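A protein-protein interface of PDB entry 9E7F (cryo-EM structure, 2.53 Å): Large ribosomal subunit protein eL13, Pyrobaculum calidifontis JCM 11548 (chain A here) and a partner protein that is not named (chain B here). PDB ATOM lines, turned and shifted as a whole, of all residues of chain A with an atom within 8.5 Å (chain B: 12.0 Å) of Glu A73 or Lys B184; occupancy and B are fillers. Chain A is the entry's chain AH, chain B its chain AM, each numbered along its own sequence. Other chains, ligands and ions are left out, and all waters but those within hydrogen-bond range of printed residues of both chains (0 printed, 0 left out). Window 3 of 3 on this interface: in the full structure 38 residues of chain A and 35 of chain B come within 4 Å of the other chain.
Of chain B, only Leu B183 comes within 4 Å of Ile A69.
Of chain B, only Lys B176, Leu B180 and Lys B184 come within 4 Å of Glu A73.
Gly A74 touches just one residue of chain B: Lys B176 (3.7 Å).
No residue of chain B comes within 4 Å of Lys A75.
No residue of chain B comes within 4 Å of Ala A76.
Of the printed residues of chain A, Ile B172 touches Val A71 (3.9 Å) and Leu A72 (3.7 Å).
Printed residues of chain A within 4 Å of Leu B175: Leu A72.
Of the printed residues of chain A, Leu B180 touches Leu A72 (3.4 Å) and Glu A73 (3.8 Å).
Of the printed residues of chain A, Leu B183 touches Arg A65 (3.5 Å), Leu A68 (3.6 Å), Ile A69 (3.9 Å) and Leu A72 (3.99 Å).
No residue of chain A comes within 4 Å of Gly B185.
The nearest printed residue of chain A that does not touch Leu B180 is Ile A69 (4.1 Å).
The backbone carbonyl oxygen of Leu B175 lies within hydrogen-bond range of the backbone NH of Leu B180 (3.1 Å).
Hydrophobic or aromatic side chains of chain B that line the printed part of chain A: Ile B172, Leu B175, Leu B180 and Leu B183.
Hydrophobic or aromatic side chains of chain A within 4 Å of the printed part of chain B: Leu A68, Ile A69, Val A71 and Leu A72.
Among the printed residues, 13 pairs touch across the chains.
Among the printed residues, pairs that only touch across the chains: Arg A65 with Leu B183 (3.5 Å), Leu A68 with Leu B183 (3.6 Å), Ile A69 with Leu B183 (3.9 Å), Val A71 with Ile B172 (3.9 Å), Leu A72 with Ile B172 (3.7 Å), Leu A72 with Leu B175 (3.4 Å), Leu A72 with Leu B180 (3.4 Å), Leu A72 with Leu B183 (3.99 Å), Glu A73 with Lys B176 (3.9 Å), Glu A73 with Leu B180 (3.8 Å) and Gly A74 with Lys B176 (3.7 Å).
The side-chain carboxylate (OE2) of Glu A73 lies within salt-bridge range of the side-chain amino group (NZ) of Lys B184 (2.9 Å).
The backbone carbonyl oxygen (O) of Leu A72 sits at hydrogen-bond distance from the side-chain amino group (NZ) of Lys B176, at 2.5 Å.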
ATOM      1  N   ARG A  65      -6.869  14.398  11.369  1.00  0.00           N
ATOM      2  CA  ARG A  65      -7.023  15.657  12.090  1.00  0.00           C
ATOM      3  C   ARG A  65      -7.397  16.795  11.149  1.00  0.00           C
ATOM      4  O   ARG A  65      -8.232  17.641  11.487  1.00  0.00           O
ATOM      5  CB  ARG A  65      -5.742  15.988  12.849  1.00  0.00           C
ATOM      6  CG  ARG A  65      -5.696  17.412  13.362  1.00  0.00           C
ATOM      7  CD  ARG A  65      -4.361  17.730  14.019  1.00  0.00           C
ATOM      8  NE  ARG A  65      -3.870  16.658  14.878  1.00  0.00           N
ATOM      9  CZ  ARG A  65      -4.461  16.237  15.989  1.00  0.00           C
ATOM     10  NH1 ARG A  65      -5.586  16.778  16.426  1.00  0.00           N
ATOM     11  NH2 ARG A  65      -3.905  15.249  16.683  1.00  0.00           N
ATOM     12  N   LYS A  66      -6.772  16.849   9.974  1.00  0.00           N
ATOM     13  CA  LYS A  66      -7.103  17.887   9.003  1.00  0.00           C
ATOM     14  C   LYS A  66      -8.530  17.730   8.506  1.00  0.00           C
ATOM     15  O   LYS A  66      -9.264  18.713   8.369  1.00  0.00           O
ATOM     16  CB  LYS A  66      -6.124  17.848   7.831  1.00  0.00           C
ATOM     17  CG  LYS A  66      -4.665  17.926   8.225  1.00  0.00           C
ATOM     18  CD  LYS A  66      -3.904  18.858   7.305  1.00  0.00           C
ATOM     19  CE  LYS A  66      -2.784  19.566   8.041  1.00  0.00           C
ATOM     20  NZ  LYS A  66      -1.537  18.762   8.077  1.00  0.00           N
ATOM     21  N   TRP A  67      -8.943  16.497   8.226  1.00  0.00           N
ATOM     22  CA  TRP A  67     -10.297  16.281   7.734  1.00  0.00           C
ATOM     23  C   TRP A  67     -11.327  16.512   8.830  1.00  0.00           C
ATOM     24  O   TRP A  67     -12.417  17.029   8.563  1.00  0.00           O
ATOM     25  CB  TRP A  67     -10.428  14.876   7.156  1.00  0.00           C
ATOM     26  CG  TRP A  67     -11.765  14.630   6.562  1.00  0.00           C
ATOM     27  CD1 TRP A  67     -12.161  14.923   5.296  1.00  0.00           C
ATOM     28  CD2 TRP A  67     -12.890  14.020   7.203  1.00  0.00           C
ATOM     29  NE1 TRP A  67     -13.465  14.547   5.107  1.00  0.00           N
ATOM     30  CE2 TRP A  67     -13.936  13.990   6.265  1.00  0.00           C
ATOM     31  CE3 TRP A  67     -13.114  13.504   8.481  1.00  0.00           C
ATOM     32  CZ2 TRP A  67     -15.187  13.466   6.562  1.00  0.00           C
ATOM     33  CZ3 TRP A  67     -14.352  12.983   8.775  1.00  0.00           C
ATOM     34  CH2 TRP A  67     -15.375  12.965   7.819  1.00  0.00           C
ATOM     35  N   LEU A  68     -10.998  16.137  10.068  1.00  0.00           N
ATOM     36  CA  LEU A  68     -11.937  16.303  11.170  1.00  0.00           C
ATOM     37  C   LEU A  68     -12.205  17.772  11.454  1.00  0.00           C
ATOM     38  O   LEU A  68     -13.312  18.141  11.858  1.00  0.00           O
ATOM     39  CB  LEU A  68     -11.403  15.616  12.422  1.00  0.00           C
ATOM     40  CG  LEU A  68     -11.641  14.117  12.551  1.00  0.00           C
ATOM     41  CD1 LEU A  68     -10.610  13.527  13.483  1.00  0.00           C
ATOM     42  CD2 LEU A  68     -13.044  13.851  13.065  1.00  0.00           C
ATOM     43  N   ILE A  69     -11.199  18.625  11.260  1.00  0.00           N
ATOM     44  CA  ILE A  69     -11.380  20.053  11.489  1.00  0.00           C
ATOM     45  C   ILE A  69     -12.328  20.648  10.456  1.00  0.00           C
ATOM     46  O   ILE A  69     -13.180  21.481  10.784  1.00  0.00           O
ATOM     47  CB  ILE A  69     -10.022  20.771  11.489  1.00  0.00           C
ATOM     48  CG1 ILE A  69      -9.357  20.634  12.856  1.00  0.00           C
ATOM     49  CG2 ILE A  69     -10.203  22.227  11.127  1.00  0.00           C
ATOM     50  CD1 ILE A  69      -7.872  20.472  12.794  1.00  0.00           C
ATOM     51  N   GLU A  70     -12.191  20.237   9.192  1.00  0.00           N
ATOM     52  CA  GLU A  70     -13.075  20.740   8.146  1.00  0.00           C
ATOM     53  C   GLU A  70     -14.514  20.307   8.387  1.00  0.00           C
ATOM     54  O   GLU A  70     -15.454  21.070   8.138  1.00  0.00           O
ATOM     55  CB  GLU A  70     -12.602  20.252   6.778  1.00  0.00           C
ATOM     56  CG  GLU A  70     -11.105  20.317   6.577  1.00  0.00           C
ATOM     57  CD  GLU A  70     -10.714  21.119   5.354  1.00  0.00           C
ATOM     58  OE1 GLU A  70     -11.616  21.621   4.652  1.00  0.00           O
ATOM     59  OE2 GLU A  70      -9.500  21.243   5.096  1.00  0.00           O
ATOM     60  N   VAL A  71     -14.706  19.075   8.858  1.00  0.00           N
ATOM     61  CA  VAL A  71     -16.049  18.582   9.140  1.00  0.00           C
ATOM     62  C   VAL A  71     -16.661  19.342  10.304  1.00  0.00           C
ATOM     63  O   VAL A  71     -17.821  19.763  10.250  1.00  0.00           O
ATOM     64  CB  VAL A  71     -16.009  17.070   9.416  1.00  0.00           C
ATOM     65  CG1 VAL A  71     -17.403  16.547   9.703  1.00  0.00           C
ATOM     66  CG2 VAL A  71     -15.381  16.350   8.251  1.00  0.00           C
ATOM     67  N   LEU A  72     -15.893  19.528  11.374  1.00  0.00           N
ATOM     68  CA  LEU A  72     -16.405  20.187  12.564  1.00  0.00           C
ATOM     69  C   LEU A  72     -16.443  21.700  12.429  1.00  0.00           C
ATOM     70  O   LEU A  72     -17.033  22.368  13.284  1.00  0.00           O
ATOM     71  CB  LEU A  72     -15.568  19.789  13.775  1.00  0.00           C
ATOM     72  CG  LEU A  72     -15.787  18.323  14.140  1.00  0.00           C
ATOM     73  CD1 LEU A  72     -14.967  17.930  15.354  1.00  0.00           C
ATOM     74  CD2 LEU A  72     -17.265  18.063  14.367  1.00  0.00           C
ATOM     75  N   GLU A  73     -15.833  22.256  11.386  1.00  0.00           N
ATOM     76  CA  GLU A  73     -15.974  23.666  11.066  1.00  0.00           C
ATOM     77  C   GLU A  73     -16.962  23.899   9.938  1.00  0.00           C
ATOM     78  O   GLU A  73     -17.009  24.997   9.379  1.00  0.00           O
ATOM     79  CB  GLU A  73     -14.618  24.271  10.718  1.00  0.00           C
ATOM     80  CG  GLU A  73     -13.707  24.439  11.912  1.00  0.00           C
ATOM     81  CD  GLU A  73     -12.551  25.362  11.623  1.00  0.00           C
ATOM     82  OE1 GLU A  73     -12.059  25.354  10.477  1.00  0.00           O
ATOM     83  OE2 GLU A  73     -12.137  26.101  12.535  1.00  0.00           O
ATOM     84  N   GLY A  74     -17.730  22.878   9.568  1.00  0.00           N
ATOM     85  CA  GLY A  74     -18.781  23.029   8.584  1.00  0.00           C
ATOM     86  C   GLY A  74     -18.287  23.304   7.180  1.00  0.00           C
ATOM     87  O   GLY A  74     -19.054  23.758   6.328  1.00  0.00           O
ATOM     88  N   LYS A  75     -17.010  23.035   6.927  1.00  0.00           N
ATOM     89  CA  LYS A  75     -16.408  23.254   5.621  1.00  0.00           C
ATOM     90  C   LYS A  75     -16.423  22.010   4.746  1.00  0.00           C
ATOM     91  O   LYS A  75     -16.023  22.087   3.580  1.00  0.00           O
ATOM     92  CB  LYS A  75     -14.970  23.745   5.785  1.00  0.00           C
ATOM     93  CG  LYS A  75     -14.857  25.163   6.291  1.00  0.00           C
ATOM     94  CD  LYS A  75     -14.088  26.008   5.308  1.00  0.00           C
ATOM     95  CE  LYS A  75     -14.839  26.111   3.996  1.00  0.00           C
ATOM     96  NZ  LYS A  75     -13.988  26.667   2.912  1.00  0.00           N
ATOM     97  N   ALA A  76     -16.870  20.873   5.271  1.00  0.00           N
ATOM     98  CA  ALA A  76     -16.893  19.632   4.517  1.00  0.00           C
ATOM     99  C   ALA A  76     -18.131  18.834   4.888  1.00  0.00           C
ATOM    100  O   ALA A  76     -18.580  18.867   6.035  1.00  0.00           O
ATOM    101  CB  ALA A  76     -15.634  18.795   4.778  1.00  0.00           C
ATOM    102  N   GLN B 168     -25.810  10.759  12.950  1.00  0.00           N
ATOM    103  CA  GLN B 168     -24.647  11.494  12.468  1.00  0.00           C
ATOM    104  C   GLN B 168     -24.827  12.994  12.640  1.00  0.00           C
ATOM    105  O   GLN B 168     -23.852  13.714  12.880  1.00  0.00           O
ATOM    106  CB  GLN B 168     -24.374  11.156  11.006  1.00  0.00           C
ATOM    107  CG  GLN B 168     -23.205  11.917  10.427  1.00  0.00           C
ATOM    108  CD  GLN B 168     -22.853  11.466   9.033  1.00  0.00           C
ATOM    109  OE1 GLN B 168     -23.344  12.015   8.051  1.00  0.00           O
ATOM    110  NE2 GLN B 168     -21.996  10.465   8.935  1.00  0.00           N
ATOM    111  N   ARG B 169     -26.059  13.487  12.497  1.00  0.00           N
ATOM    112  CA  ARG B 169     -26.321  14.904  12.732  1.00  0.00           C
ATOM    113  C   ARG B 169     -26.042  15.285  14.179  1.00  0.00           C
ATOM    114  O   ARG B 169     -25.446  16.332  14.448  1.00  0.00           O
ATOM    115  CB  ARG B 169     -27.766  15.238  12.365  1.00  0.00           C
ATOM    116  CG  ARG B 169     -27.941  15.782  10.963  1.00  0.00           C
ATOM    117  CD  ARG B 169     -28.885  14.925  10.141  1.00  0.00           C
ATOM    118  NE  ARG B 169     -30.084  14.555  10.880  1.00  0.00           N
ATOM    119  CZ  ARG B 169     -31.077  13.833  10.379  1.00  0.00           C
ATOM    120  NH1 ARG B 169     -31.049  13.395   9.132  1.00  0.00           N
ATOM    121  NH2 ARG B 169     -32.125  13.549  11.147  1.00  0.00           N
ATOM    122  N   LEU B 171     -24.161  13.577  16.407  1.00  0.00           N
ATOM    123  CA  LEU B 171     -22.764  13.368  16.770  1.00  0.00           C
ATOM    124  C   LEU B 171     -21.895  14.528  16.309  1.00  0.00           C
ATOM    125  O   LEU B 171     -20.979  14.951  17.023  1.00  0.00           O
ATOM    126  CB  LEU B 171     -22.250  12.055  16.180  1.00  0.00           C
ATOM    127  CG  LEU B 171     -20.729  11.902  16.197  1.00  0.00           C
ATOM    128  CD1 LEU B 171     -20.229  11.655  17.603  1.00  0.00           C
ATOM    129  CD2 LEU B 171     -20.290  10.792  15.274  1.00  0.00           C
ATOM    130  N   ILE B 172     -22.156  15.044  15.107  1.00  0.00           N
ATOM    131  CA  ILE B 172     -21.375  16.159  14.583  1.00  0.00           C
ATOM    132  C   ILE B 172     -21.616  17.409  15.411  1.00  0.00           C
ATOM    133  O   ILE B 172     -20.705  18.216  15.627  1.00  0.00           O
ATOM    134  CB  ILE B 172     -21.710  16.394  13.100  1.00  0.00           C
ATOM    135  CG1 ILE B 172     -20.880  15.469  12.210  1.00  0.00           C
ATOM    136  CG2 ILE B 172     -21.508  17.857  12.734  1.00  0.00           C
ATOM    137  CD1 ILE B 172     -21.029  15.752  10.741  1.00  0.00           C
ATOM    138  N   GLU B 173     -22.851  17.593  15.878  1.00  0.00           N
ATOM    139  CA  GLU B 173     -23.177  18.724  16.737  1.00  0.00           C
ATOM    140  C   GLU B 173     -22.404  18.661  18.048  1.00  0.00           C
ATOM    141  O   GLU B 173     -21.897  19.678  18.530  1.00  0.00           O
ATOM    142  CB  GLU B 173     -24.680  18.744  16.996  1.00  0.00           C
ATOM    143  CG  GLU B 173     -25.220  20.043  17.538  1.00  0.00           C
ATOM    144  CD  GLU B 173     -26.456  19.840  18.391  1.00  0.00           C
ATOM    145  OE1 GLU B 173     -27.367  19.105  17.956  1.00  0.00           O
ATOM    146  OE2 GLU B 173     -26.514  20.410  19.499  1.00  0.00           O
ATOM    147  N   HIS B 174     -22.293  17.469  18.627  1.00  0.00           N
ATOM    148  CA  HIS B 174     -21.587  17.296  19.890  1.00  0.00           C
ATOM    149  C   HIS B 174     -20.076  17.381  19.713  1.00  0.00           C
ATOM    150  O   HIS B 174     -19.375  17.882  20.597  1.00  0.00           O
ATOM    151  CB  HIS B 174     -21.987  15.962  20.515  1.00  0.00           C
ATOM    152  CG  HIS B 174     -21.291  15.659  21.802  1.00  0.00           C
ATOM    153  ND1 HIS B 174     -21.784  16.055  23.025  1.00  0.00           N
ATOM    154  CD2 HIS B 174     -20.151  14.975  22.058  1.00  0.00           C
ATOM    155  CE1 HIS B 174     -20.969  15.643  23.978  1.00  0.00           C
ATOM    156  NE2 HIS B 174     -19.970  14.985  23.419  1.00  0.00           N
ATOM    157  N   LEU B 175     -19.553  16.886  18.587  1.00  0.00           N
ATOM    158  CA  LEU B 175     -18.108  16.887  18.380  1.00  0.00           C
ATOM    159  C   LEU B 175     -17.582  18.288  18.104  1.00  0.00           C
ATOM    160  O   LEU B 175     -16.421  18.586  18.403  1.00  0.00           O
ATOM    161  CB  LEU B 175     -17.736  15.945  17.238  1.00  0.00           C
ATOM    162  CG  LEU B 175     -17.623  14.458  17.574  1.00  0.00           C
ATOM    163  CD1 LEU B 175     -17.060  13.686  16.393  1.00  0.00           C
ATOM    164  CD2 LEU B 175     -16.775  14.242  18.810  1.00  0.00           C
ATOM    165  N   LYS B 176     -18.412  19.153  17.517  1.00  0.00           N
ATOM    166  CA  LYS B 176     -18.004  20.534  17.273  1.00  0.00           C
ATOM    167  C   LYS B 176     -17.725  21.263  18.579  1.00  0.00           C
ATOM    168  O   LYS B 176     -16.750  22.013  18.690  1.00  0.00           O
ATOM    169  CB  LYS B 176     -19.084  21.271  16.482  1.00  0.00           C
ATOM    170  CG  LYS B 176     -19.095  20.966  15.007  1.00  0.00           C
ATOM    171  CD  LYS B 176     -20.484  21.117  14.431  1.00  0.00           C
ATOM    172  CE  LYS B 176     -20.433  21.680  13.027  1.00  0.00           C
ATOM    173  NZ  LYS B 176     -19.423  22.763  12.912  1.00  0.00           N
ATOM    174  N   LYS B 177     -18.575  21.053  19.579  1.00  0.00           N
ATOM    175  CA  LYS B 177     -18.441  21.774  20.836  1.00  0.00           C
ATOM    176  C   LYS B 177     -17.423  21.135  21.772  1.00  0.00           C
ATOM    177  O   LYS B 177     -16.990  21.778  22.732  1.00  0.00           O
ATOM    178  CB  LYS B 177     -19.801  21.861  21.529  1.00  0.00           C
ATOM    179  CG  LYS B 177     -19.933  20.898  22.685  1.00  0.00           C
ATOM    180  CD  LYS B 177     -21.297  20.942  23.336  1.00  0.00           C
ATOM    181  CE  LYS B 177     -21.229  20.348  24.735  1.00  0.00           C
ATOM    182  NZ  LYS B 177     -22.457  19.593  25.100  1.00  0.00           N
ATOM    183  N   THR B 178     -17.028  19.887  21.522  1.00  0.00           N
ATOM    184  CA  THR B 178     -16.208  19.146  22.471  1.00  0.00           C
ATOM    185  C   THR B 178     -14.905  18.609  21.899  1.00  0.00           C
ATOM    186  O   THR B 178     -14.011  18.262  22.676  1.00  0.00           O
ATOM    187  CB  THR B 178     -17.005  17.972  23.055  1.00  0.00           C
ATOM    188  OG1 THR B 178     -17.597  17.218  21.990  1.00  0.00           O
ATOM    189  CG2 THR B 178     -18.092  18.471  23.985  1.00  0.00           C
ATOM    190  N   LEU B 179     -14.764  18.524  20.579  1.00  0.00           N
ATOM    191  CA  LEU B 179     -13.578  17.899  20.006  1.00  0.00           C
ATOM    192  C   LEU B 179     -12.833  18.863  19.097  1.00  0.00           C
ATOM    193  O   LEU B 179     -11.619  18.738  18.911  1.00  0.00           O
ATOM    194  CB  LEU B 179     -13.960  16.635  19.232  1.00  0.00           C
ATOM    195  CG  LEU B 179     -12.821  15.904  18.529  1.00  0.00           C
ATOM    196  CD1 LEU B 179     -11.856  15.334  19.545  1.00  0.00           C
ATOM    197  CD2 LEU B 179     -13.367  14.808  17.638  1.00  0.00           C
ATOM    198  N   LEU B 180     -13.561  19.811  18.517  1.00  0.00           N
ATOM    199  CA  LEU B 180     -12.947  20.803  17.637  1.00  0.00           C
ATOM    200  C   LEU B 180     -11.903  21.668  18.330  1.00  0.00           C
ATOM    201  O   LEU B 180     -10.855  21.932  17.715  1.00  0.00           O
ATOM    202  CB  LEU B 180     -14.040  21.662  17.001  1.00  0.00           C
ATOM    203  CG  LEU B 180     -13.544  22.657  15.958  1.00  0.00           C
ATOM    204  CD1 LEU B 180     -12.827  21.928  14.837  1.00  0.00           C
ATOM    205  CD2 LEU B 180     -14.701  23.481  15.424  1.00  0.00           C
ATOM    206  N   PRO B 181     -12.130  22.190  19.545  1.00  0.00           N
ATOM    207  CA  PRO B 181     -11.054  22.928  20.230  1.00  0.00           C
ATOM    208  C   PRO B 181      -9.796  22.118  20.462  1.00  0.00           C
ATOM    209  O   PRO B 181      -8.690  22.667  20.379  1.00  0.00           O
ATOM    210  CB  PRO B 181     -11.702  23.324  21.562  1.00  0.00           C
ATOM    211  CG  PRO B 181     -13.136  23.431  21.256  1.00  0.00           C
ATOM    212  CD  PRO B 181     -13.429  22.392  20.219  1.00  0.00           C
ATOM    213  N   LYS B 182      -9.927  20.825  20.749  1.00  0.00           N
ATOM    214  CA  LYS B 182      -8.745  20.012  21.000  1.00  0.00           C
ATOM    215  C   LYS B 182      -8.000  19.763  19.692  1.00  0.00           C
ATOM    216  O   LYS B 182      -6.765  19.796  19.659  1.00  0.00           O
ATOM    217  CB  LYS B 182      -9.179  18.706  21.688  1.00  0.00           C
ATOM    218  CG  LYS B 182      -8.261  17.453  21.715  1.00  0.00           C
ATOM    219  CD  LYS B 182      -6.750  17.695  21.807  1.00  0.00           C
ATOM    220  CE  LYS B 182      -6.313  17.824  23.248  1.00  0.00           C
ATOM    221  NZ  LYS B 182      -6.538  16.562  23.984  1.00  0.00           N
ATOM    222  N   LEU B 183      -8.735  19.506  18.608  1.00  0.00           N
ATOM    223  CA  LEU B 183      -8.103  19.246  17.320  1.00  0.00           C
ATOM    224  C   LEU B 183      -7.352  20.470  16.816  1.00  0.00           C
ATOM    225  O   LEU B 183      -6.202  20.367  16.377  1.00  0.00           O
ATOM    226  CB  LEU B 183      -9.157  18.814  16.302  1.00  0.00           C
ATOM    227  CG  LEU B 183      -9.951  17.564  16.663  1.00  0.00           C
ATOM    228  CD1 LEU B 183     -11.038  17.302  15.635  1.00  0.00           C
ATOM    229  CD2 LEU B 183      -9.015  16.388  16.791  1.00  0.00           C
ATOM    230  N   LYS B 184      -7.990  21.642  16.881  1.00  0.00           N
ATOM    231  CA  LYS B 184      -7.352  22.864  16.403  1.00  0.00           C
ATOM    232  C   LYS B 184      -6.152  23.229  17.262  1.00  0.00           C
ATOM    233  O   LYS B 184      -5.107  23.637  16.743  1.00  0.00           O
ATOM    234  CB  LYS B 184      -8.365  24.008  16.380  1.00  0.00           C
ATOM    235  CG  LYS B 184      -9.035  24.208  15.040  1.00  0.00           C
ATOM    236  CD  LYS B 184      -9.735  25.548  14.957  1.00  0.00           C
ATOM    237  CE  LYS B 184     -11.210  25.438  15.330  1.00  0.00           C
ATOM    238  NZ  LYS B 184     -11.877  26.772  15.374  1.00  0.00           N
ATOM    239  N   GLY B 185      -6.280  23.086  18.576  1.00  0.00           N
ATOM    240  CA  GLY B 185      -5.183  23.367  19.481  1.00  0.00           C
ATOM    241  C   GLY B 185      -4.021  22.411  19.299  1.00  0.00           C
ATOM    242  O   GLY B 185      -4.008  21.327  19.876  1.00  0.00           O
